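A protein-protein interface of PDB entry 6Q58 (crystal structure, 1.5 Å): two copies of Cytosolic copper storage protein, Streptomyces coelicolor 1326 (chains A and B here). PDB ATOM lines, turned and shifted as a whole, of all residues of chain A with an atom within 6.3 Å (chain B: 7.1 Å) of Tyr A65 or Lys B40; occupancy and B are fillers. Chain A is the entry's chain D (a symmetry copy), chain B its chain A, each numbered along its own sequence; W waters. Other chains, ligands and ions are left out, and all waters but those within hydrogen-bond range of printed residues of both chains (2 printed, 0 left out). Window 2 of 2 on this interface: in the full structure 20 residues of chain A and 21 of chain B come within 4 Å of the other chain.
NZ of Lys B40 is in salt-bridge range of OD2 of Asp A66 (2.8 Å).
O of Lys B40 sits at hydrogen-bond distance from OG1 of Thr B44, at 2.8 Å.
The backbone carbonyl oxygen (O) of Tyr A65 is in hydrogen-bond range of the side-chain hydroxyl (OG1) of Thr A63 (3.2 Å).
The side-chain amide oxygen (OD1) of Asn A68 sits close to the side-chain carboxylate (OD1) of Asp A66, 2.6 Å away.
Among the printed residues, pairs that only touch across the chains: Tyr A65 with Lys B40, Val A69 with Ala B83, Thr A63 with Arg B43 and Asp A66 with Ala B83.
No residue of chain B comes within 4 Å of Gly A64.
Tyr A65 touches just one residue of chain B: Lys B40 (3.1 Å).
Printed residues of chain B within 4 Å of Asp A66: Lys B40 and Ala B83.
Of the printed residues of chain B, Val A69 touches Ala B83 (3.5 Å).
Of the printed residues of chain A, Lys B40 touches Tyr A65 and Asp A66.
Printed residues of chain A within 4 Å of Arg B43: Thr A63 (3.6 Å).
Of the printed residues of chain A, Ala B83 touches Asp A66 (3.7 Å) and Val A69 (3.5 Å).
The nearest residue of chain A that does not touch Lys B40 is Thr A63 (4.5 Å).
The nearest printed residue of chain A that does not touch Ala B83 is Asn A68 (4.7 Å).
Of the 9 printed residues of chain A, 4 touch a printed residue of chain B.
Hydrophobic or aromatic side chains of chain A that line the printed part of chain B: Tyr A65 and Val A69.
Along chain A the printed residues that touch a printed residue of chain B span positions 63 to 69.
Of the 18 printed residues of chain B, 3 touch a printed residue of chain A.
Hydrophobic or aromatic side chains of chain B that line the printed part of chain A: Ala B83.
Among the printed residues, Asp or Glu carboxylates within 4 Å of a Lys or Arg side-chain nitrogen of the other chain: Asp A66 with Lys B40.
No position is printed for both chains.
Water W1 bridges the side-chain carboxylate (OD2) of Asp B47 (2.7 Å) and the backbone NH (N) of His A62 (3.5 Å).
Water W2 lies within hydrogen-bond range of the backbone carbonyl oxygen of Ala B83 and the side-chain carboxylate of Asp A66.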
ATOM      1  N   HIS A  62     -10.857  19.764   1.786  1.00  0.00           N
ATOM      2  CA  HIS A  62     -11.974  20.017   2.708  1.00  0.00           C
ATOM      3  C   HIS A  62     -13.234  20.393   1.916  1.00  0.00           C
ATOM      4  O   HIS A  62     -13.184  21.224   1.038  1.00  0.00           O
ATOM      5  CB  HIS A  62     -11.594  21.137   3.639  1.00  0.00           C
ATOM      6  CG  HIS A  62     -12.693  21.538   4.569  1.00  0.00           C
ATOM      7  ND1 HIS A  62     -12.983  20.847   5.720  1.00  0.00           N
ATOM      8  CD2 HIS A  62     -13.590  22.552   4.500  1.00  0.00           C
ATOM      9  CE1 HIS A  62     -14.009  21.415   6.329  1.00  0.00           C
ATOM     10  NE2 HIS A  62     -14.382  22.465   5.618  1.00  0.00           N
ATOM     11  N   THR A  63     -14.323  19.721   2.236  1.00  0.00           N
ATOM     12  CA  THR A  63     -15.639  20.013   1.640  1.00  0.00           C
ATOM     13  C   THR A  63     -16.712  20.490   2.633  1.00  0.00           C
ATOM     14  O   THR A  63     -17.813  20.841   2.221  1.00  0.00           O
ATOM     15  CB  THR A  63     -16.223  18.751   0.976  1.00  0.00           C
ATOM     16  OG1 THR A  63     -16.463  17.778   1.996  1.00  0.00           O
ATOM     17  CG2 THR A  63     -15.253  18.201  -0.058  1.00  0.00           C
ATOM     18  N   GLY A  64     -16.406  20.487   3.906  1.00  0.00           N
ATOM     19  CA  GLY A  64     -17.351  21.055   4.882  1.00  0.00           C
ATOM     20  C   GLY A  64     -18.095  19.953   5.597  1.00  0.00           C
ATOM     21  O   GLY A  64     -18.214  19.948   6.840  1.00  0.00           O
ATOM     22  N   TYR A  65     -18.658  19.021   4.848  1.00  0.00           N
ATOM     23  CA  TYR A  65     -19.118  17.776   5.530  1.00  0.00           C
ATOM     24  C   TYR A  65     -17.883  16.934   5.793  1.00  0.00           C
ATOM     25  O   TYR A  65     -16.896  16.962   5.066  1.00  0.00           O
ATOM     26  CB  TYR A  65     -20.265  17.060   4.823  1.00  0.00           C
ATOM     27  CG  TYR A  65     -19.895  16.296   3.596  1.00  0.00           C
ATOM     28  CD1 TYR A  65     -19.767  16.950   2.388  1.00  0.00           C
ATOM     29  CD2 TYR A  65     -19.738  14.902   3.619  1.00  0.00           C
ATOM     30  CE1 TYR A  65     -19.478  16.258   1.213  1.00  0.00           C
ATOM     31  CE2 TYR A  65     -19.441  14.202   2.459  1.00  0.00           C
ATOM     32  CZ  TYR A  65     -19.310  14.888   1.260  1.00  0.00           C
ATOM     33  OH  TYR A  65     -19.019  14.218   0.099  1.00  0.00           O
ATOM     34  N   ASP A  66     -17.869  16.252   6.936  1.00  0.00           N
ATOM     35  CA  ASP A  66     -16.673  15.534   7.493  1.00  0.00           C
ATOM     36  C   ASP A  66     -15.612  16.535   8.009  1.00  0.00           C
ATOM     37  O   ASP A  66     -14.387  16.341   7.973  1.00  0.00           O
ATOM     38  CB  ASP A  66     -16.057  14.504   6.512  1.00  0.00           C
ATOM     39  CG  ASP A  66     -15.670  13.204   7.173  1.00  0.00           C
ATOM     40  OD1 ASP A  66     -15.141  13.235   8.282  1.00  0.00           O
ATOM     41  OD2 ASP A  66     -15.897  12.119   6.570  1.00  0.00           O
ATOM     42  N   ALA A  67     -16.137  17.612   8.554  1.00  0.00           N
ATOM     43  CA  ALA A  67     -15.370  18.573   9.336  1.00  0.00           C
ATOM     44  C   ALA A  67     -14.618  17.947  10.513  1.00  0.00           C
ATOM     45  O   ALA A  67     -13.673  18.530  11.026  1.00  0.00           O
ATOM     46  CB  ALA A  67     -16.321  19.661   9.851  1.00  0.00           C
ATOM     47  N   ASN A  68     -15.046  16.784  11.008  1.00  0.00           N
ATOM     48  CA  ASN A  68     -14.315  16.084  12.059  1.00  0.00           C
ATOM     49  C   ASN A  68     -12.891  15.708  11.620  1.00  0.00           C
ATOM     50  O   ASN A  68     -11.978  15.788  12.447  1.00  0.00           O
ATOM     51  CB  ASN A  68     -15.079  14.887  12.630  1.00  0.00           C
ATOM     52  CG  ASN A  68     -15.471  13.871  11.590  1.00  0.00           C
ATOM     53  OD1 ASN A  68     -16.061  14.225  10.554  1.00  0.00           O
ATOM     54  ND2 ASN A  68     -15.174  12.581  11.847  1.00  0.00           N
ATOM     55  N   VAL A  69     -12.699  15.350  10.359  1.00  0.00           N
ATOM     56  CA  VAL A  69     -11.363  15.088   9.840  1.00  0.00           C
ATOM     57  C   VAL A  69     -10.517  16.357   9.861  1.00  0.00           C
ATOM     58  O   VAL A  69      -9.413  16.368  10.400  1.00  0.00           O
ATOM     59  CB  VAL A  69     -11.376  14.482   8.430  1.00  0.00           C
ATOM     60  CG1 VAL A  69      -9.975  14.439   7.806  1.00  0.00           C
ATOM     61  CG2 VAL A  69     -11.973  13.085   8.488  1.00  0.00           C
ATOM     62  N   THR A  70     -11.053  17.398   9.254  1.00  0.00           N
ATOM     63  CA  THR A  70     -10.367  18.683   9.179  1.00  0.00           C
ATOM     64  C   THR A  70     -10.014  19.198  10.577  1.00  0.00           C
ATOM     65  O   THR A  70      -8.878  19.593  10.796  1.00  0.00           O
ATOM     66  CB  THR A  70     -11.206  19.696   8.384  1.00  0.00           C
ATOM     67  OG1 THR A  70     -11.434  19.187   7.073  1.00  0.00           O
ATOM     68  CG2 THR A  70     -10.524  21.007   8.265  1.00  0.00           C
ATOM     69  N   VAL B  35     -17.029   7.350 -11.287  1.00  0.00           N
ATOM     70  CA  VAL B  35     -16.163   8.277 -10.529  1.00  0.00           C
ATOM     71  C   VAL B  35     -16.876   9.487  -9.917  1.00  0.00           C
ATOM     72  O   VAL B  35     -16.569   9.869  -8.794  1.00  0.00           O
ATOM     73  CB  VAL B  35     -14.938   8.733 -11.366  1.00  0.00           C
ATOM     74  CG1 VAL B  35     -15.338   9.455 -12.640  1.00  0.00           C
ATOM     75  CG2 VAL B  35     -14.017   9.623 -10.544  1.00  0.00           C
ATOM     76  N   ALA B  36     -17.854  10.064 -10.606  1.00  0.00           N
ATOM     77  CA  ALA B  36     -18.584  11.214 -10.044  1.00  0.00           C
ATOM     78  C   ALA B  36     -19.284  10.913  -8.721  1.00  0.00           C
ATOM     79  O   ALA B  36     -19.488  11.822  -7.906  1.00  0.00           O
ATOM     80  CB  ALA B  36     -19.579  11.770 -11.049  1.00  0.00           C
ATOM     81  N   ASP B  37     -19.627   9.648  -8.497  1.00  0.00           N
ATOM     82  CA  ASP B  37     -20.255   9.192  -7.261  1.00  0.00           C
ATOM     83  C   ASP B  37     -19.262   8.793  -6.162  1.00  0.00           C
ATOM     84  O   ASP B  37     -19.675   8.444  -5.048  1.00  0.00           O
ATOM     85  CB  ASP B  37     -21.155   7.982  -7.543  1.00  0.00           C
ATOM     86  CG  ASP B  37     -22.262   8.282  -8.547  1.00  0.00           C
ATOM     87  OD1 ASP B  37     -22.748   9.427  -8.588  1.00  0.00           O
ATOM     88  OD2 ASP B  37     -22.652   7.348  -9.292  1.00  0.00           O
ATOM     89  N   LEU B  38     -17.966   8.860  -6.461  1.00  0.00           N
ATOM     90  CA  LEU B  38     -16.930   8.345  -5.571  1.00  0.00           C
ATOM     91  C   LEU B  38     -15.977   9.452  -5.129  1.00  0.00           C
ATOM     92  O   LEU B  38     -14.891   9.147  -4.623  1.00  0.00           O
ATOM     93  CB  LEU B  38     -16.142   7.256  -6.314  1.00  0.00           C
ATOM     94  CG  LEU B  38     -16.950   6.008  -6.670  1.00  0.00           C
ATOM     95  CD1 LEU B  38     -16.137   5.120  -7.599  1.00  0.00           C
ATOM     96  CD2 LEU B  38     -17.351   5.241  -5.444  1.00  0.00           C
ATOM     97  N   THR B  39     -16.336  10.715  -5.330  1.00  0.00           N
ATOM     98  CA  THR B  39     -15.388  11.804  -5.079  1.00  0.00           C
ATOM     99  C   THR B  39     -15.067  11.966  -3.588  1.00  0.00           C
ATOM    100  O   THR B  39     -13.921  12.261  -3.240  1.00  0.00           O
ATOM    101  CB  THR B  39     -15.864  13.130  -5.656  1.00  0.00           C
ATOM    102  OG1 THR B  39     -17.136  13.455  -5.096  1.00  0.00           O
ATOM    103  CG2 THR B  39     -15.977  13.050  -7.153  1.00  0.00           C
ATOM    104  N   LYS B  40     -16.036  11.772  -2.704  1.00  0.00           N
ATOM    105  CA  LYS B  40     -15.743  11.813  -1.272  1.00  0.00           C
ATOM    106  C   LYS B  40     -14.842  10.656  -0.846  1.00  0.00           C
ATOM    107  O   LYS B  40     -13.934  10.825  -0.024  1.00  0.00           O
ATOM    108  CB  LYS B  40     -17.020  11.859  -0.422  1.00  0.00           C
ATOM    109  CG  LYS B  40     -16.745  12.008   1.077  1.00  0.00           C
ATOM    110  CD  LYS B  40     -15.791  13.123   1.475  1.00  0.00           C
ATOM    111  CE  LYS B  40     -15.908  13.404   2.964  1.00  0.00           C
ATOM    112  NZ  LYS B  40     -15.759  12.175   3.802  1.00  0.00           N
ATOM    113  N   CYS B  41     -15.069   9.479  -1.422  1.00  0.00           N
ATOM    114  CA  CYS B  41     -14.206   8.336  -1.187  1.00  0.00           C
ATOM    115  C   CYS B  41     -12.754   8.661  -1.572  1.00  0.00           C
ATOM    116  O   CYS B  41     -11.830   8.457  -0.775  1.00  0.00           O
ATOM    117  CB  CYS B  41     -14.715   7.128  -1.949  1.00  0.00           C
ATOM    118  SG  CYS B  41     -13.740   5.703  -1.516  1.00  0.00           S
ATOM    119  N   ILE B  42     -12.571   9.175  -2.771  1.00  0.00           N
ATOM    120  CA  ILE B  42     -11.249   9.554  -3.261  1.00  0.00           C
ATOM    121  C   ILE B  42     -10.604  10.564  -2.326  1.00  0.00           C
ATOM    122  O   ILE B  42      -9.442  10.358  -1.925  1.00  0.00           O
ATOM    123  CB  ILE B  42     -11.304  10.103  -4.698  1.00  0.00           C
ATOM    124  CG1 ILE B  42     -11.664   8.971  -5.661  1.00  0.00           C
ATOM    125  CG2 ILE B  42      -9.982  10.747  -5.116  1.00  0.00           C
ATOM    126  CD1 ILE B  42     -12.283   9.464  -6.930  1.00  0.00           C
ATOM    127  N   ARG B  43     -11.334  11.632  -1.978  1.00  0.00           N
ATOM    128  CA  ARG B  43     -10.755  12.655  -1.118  1.00  0.00           C
ATOM    129  C   ARG B  43     -10.347  12.068   0.216  1.00  0.00           C
ATOM    130  O   ARG B  43      -9.243  12.362   0.713  1.00  0.00           O
ATOM    131  CB  ARG B  43     -11.749  13.793  -0.864  1.00  0.00           C
ATOM    132  CG  ARG B  43     -12.018  14.703  -2.019  1.00  0.00           C
ATOM    133  CD  ARG B  43     -13.202  15.590  -1.654  1.00  0.00           C
ATOM    134  NE  ARG B  43     -13.723  16.383  -2.751  1.00  0.00           N
ATOM    135  CZ  ARG B  43     -13.190  17.504  -3.205  1.00  0.00           C
ATOM    136  NH1 ARG B  43     -12.066  18.034  -2.666  1.00  0.00           N
ATOM    137  NH2 ARG B  43     -13.796  18.145  -4.192  1.00  0.00           N
ATOM    138  N   THR B  44     -11.212  11.278   0.826  1.00  0.00           N
ATOM    139  CA  THR B  44     -10.950  10.747   2.144  1.00  0.00           C
ATOM    140  C   THR B  44      -9.820   9.705   2.105  1.00  0.00           C
ATOM    141  O   THR B  44      -9.011   9.603   3.042  1.00  0.00           O
ATOM    142  CB  THR B  44     -12.241  10.248   2.819  1.00  0.00           C
ATOM    143  OG1 THR B  44     -13.259  11.279   2.706  1.00  0.00           O
ATOM    144  CG2 THR B  44     -12.002  10.007   4.251  1.00  0.00           C
ATOM    145  N   ASP B  45      -9.753   8.941   1.025  1.00  0.00           N
ATOM    146  CA  ASP B  45      -8.614   8.020   0.787  1.00  0.00           C
ATOM    147  C   ASP B  45      -7.311   8.774   0.805  1.00  0.00           C
ATOM    148  O   ASP B  45      -6.347   8.303   1.421  1.00  0.00           O
ATOM    149  CB  ASP B  45      -8.703   7.347  -0.584  1.00  0.00           C
ATOM    150  CG  ASP B  45      -9.780   6.294  -0.678  1.00  0.00           C
ATOM    151  OD1 ASP B  45     -10.229   5.733   0.335  1.00  0.00           O
ATOM    152  OD2 ASP B  45     -10.098   6.044  -1.872  1.00  0.00           O
ATOM    153  N   MET B  46      -7.279   9.914   0.125  1.00  0.00           N
ATOM    154  CA  MET B  46      -6.048  10.695   0.034  1.00  0.00           C
ATOM    155  C   MET B  46      -5.682  11.269   1.378  1.00  0.00           C
ATOM    156  O   MET B  46      -4.518  11.233   1.763  1.00  0.00           O
ATOM    157  CB  MET B  46      -6.152  11.761  -1.026  1.00  0.00           C
ATOM    158  CG  MET B  46      -6.101  11.120  -2.440  1.00  0.00           C
ATOM    159  SD  MET B  46      -5.014   9.660  -2.597  1.00  0.00           S
ATOM    160  CE  MET B  46      -3.338  10.247  -2.254  1.00  0.00           C
ATOM    161  N   ASP B  47      -6.658  11.776   2.098  1.00  0.00           N
ATOM    162  CA  ASP B  47      -6.410  12.296   3.477  1.00  0.00           C
ATOM    163  C   ASP B  47      -5.847  11.190   4.361  1.00  0.00           C
ATOM    164  O   ASP B  47      -4.867  11.385   5.107  1.00  0.00           O
ATOM    165  CB  ASP B  47      -7.680  12.840   4.147  1.00  0.00           C
ATOM    166  CG  ASP B  47      -8.287  14.036   3.443  1.00  0.00           C
ATOM    167  OD1 ASP B  47      -7.611  14.751   2.699  1.00  0.00           O
ATOM    168  OD2 ASP B  47      -9.523  14.269   3.624  1.00  0.00           O
ATOM    169  N   ALA B  83     -13.088   7.821   9.473  1.00  0.00           N
ATOM    170  CA  ALA B  83     -13.830   8.486   8.427  1.00  0.00           C
ATOM    171  C   ALA B  83     -13.653   7.808   7.084  1.00  0.00           C
ATOM    172  O   ALA B  83     -14.615   7.647   6.329  1.00  0.00           O
ATOM    173  CB  ALA B  83     -13.433   9.950   8.331  1.00  0.00           C
ATOM    174  N   CYS B  84     -12.419   7.421   6.766  1.00  0.00           N
ATOM    175  CA  CYS B  84     -12.154   6.800   5.481  1.00  0.00           C
ATOM    176  C   CYS B  84     -12.835   5.428   5.432  1.00  0.00           C
ATOM    177  O   CYS B  84     -13.455   5.086   4.419  1.00  0.00           O
ATOM    178  CB  CYS B  84     -10.650   6.676   5.252  1.00  0.00           C
ATOM    179  SG  CYS B  84     -10.228   6.184   3.566  1.00  0.00           S
ATOM    180  N   GLU B  87     -16.551   5.833   4.719  1.00  0.00           N
ATOM    181  CA  GLU B  87     -16.897   6.207   3.348  1.00  0.00           C
ATOM    182  C   GLU B  87     -16.656   5.034   2.395  1.00  0.00           C
ATOM    183  O   GLU B  87     -17.495   4.725   1.551  1.00  0.00           O
ATOM    184  CB  GLU B  87     -16.121   7.453   2.910  1.00  0.00           C
ATOM    185  CG  GLU B  87     -16.478   7.981   1.547  1.00  0.00           C
ATOM    186  CD  GLU B  87     -17.949   8.429   1.391  1.00  0.00           C
ATOM    187  OE1 GLU B  87     -18.618   8.745   2.401  1.00  0.00           O
ATOM    188  OE2 GLU B  87     -18.413   8.486   0.229  1.00  0.00           O
ATOM    189  N   ARG B  90     -19.444   2.408   2.464  1.00  0.00           N
ATOM    190  CA  ARG B  90     -20.638   2.759   1.666  1.00  0.00           C
ATOM    191  C   ARG B  90     -20.634   2.128   0.284  1.00  0.00           C
ATOM    192  O   ARG B  90     -21.699   1.850  -0.285  1.00  0.00           O
ATOM    193  CB  ARG B  90     -20.803   4.270   1.450  1.00  0.00           C
ATOM    194  CG  ARG B  90     -20.886   5.117   2.668  1.00  0.00           C
ATOM    195  CD  ARG B  90     -20.993   6.603   2.257  1.00  0.00           C
ATOM    196  NE  ARG B  90     -22.270   6.916   1.607  1.00  0.00           N
ATOM    197  CZ  ARG B  90     -23.283   7.644   2.126  1.00  0.00           C
ATOM    198  NH1 ARG B  90     -23.230   8.194   3.341  1.00  0.00           N
ATOM    199  NH2 ARG B  90     -24.387   7.824   1.408  1.00  0.00           N
ATOM    200  N   HIS B  91     -19.430   1.945  -0.268  1.00  0.00           N
ATOM    201  CA  HIS B  91     -19.231   1.476  -1.628  1.00  0.00           C
ATOM    202  C   HIS B  91     -18.725   0.045  -1.709  1.00  0.00           C
ATOM    203  O   HIS B  91     -18.493  -0.454  -2.811  1.00  0.00           O
ATOM    204  CB  HIS B  91     -18.248   2.410  -2.333  1.00  0.00           C
ATOM    205  CG  HIS B  91     -18.745   3.807  -2.419  1.00  0.00           C
ATOM    206  ND1 HIS B  91     -18.153   4.865  -1.748  1.00  0.00           N
ATOM    207  CD2 HIS B  91     -19.823   4.315  -3.059  1.00  0.00           C
ATOM    208  CE1 HIS B  91     -18.846   5.961  -1.989  1.00  0.00           C
ATOM    209  NE2 HIS B  91     -19.859   5.659  -2.784  1.00  0.00           N
HETATM  210  O   HOH W   1     -10.191  16.855   3.554  1.00  0.00           O
HETATM  211  O   HOH W   2     -16.846   9.137   6.597  1.00  0.00           O
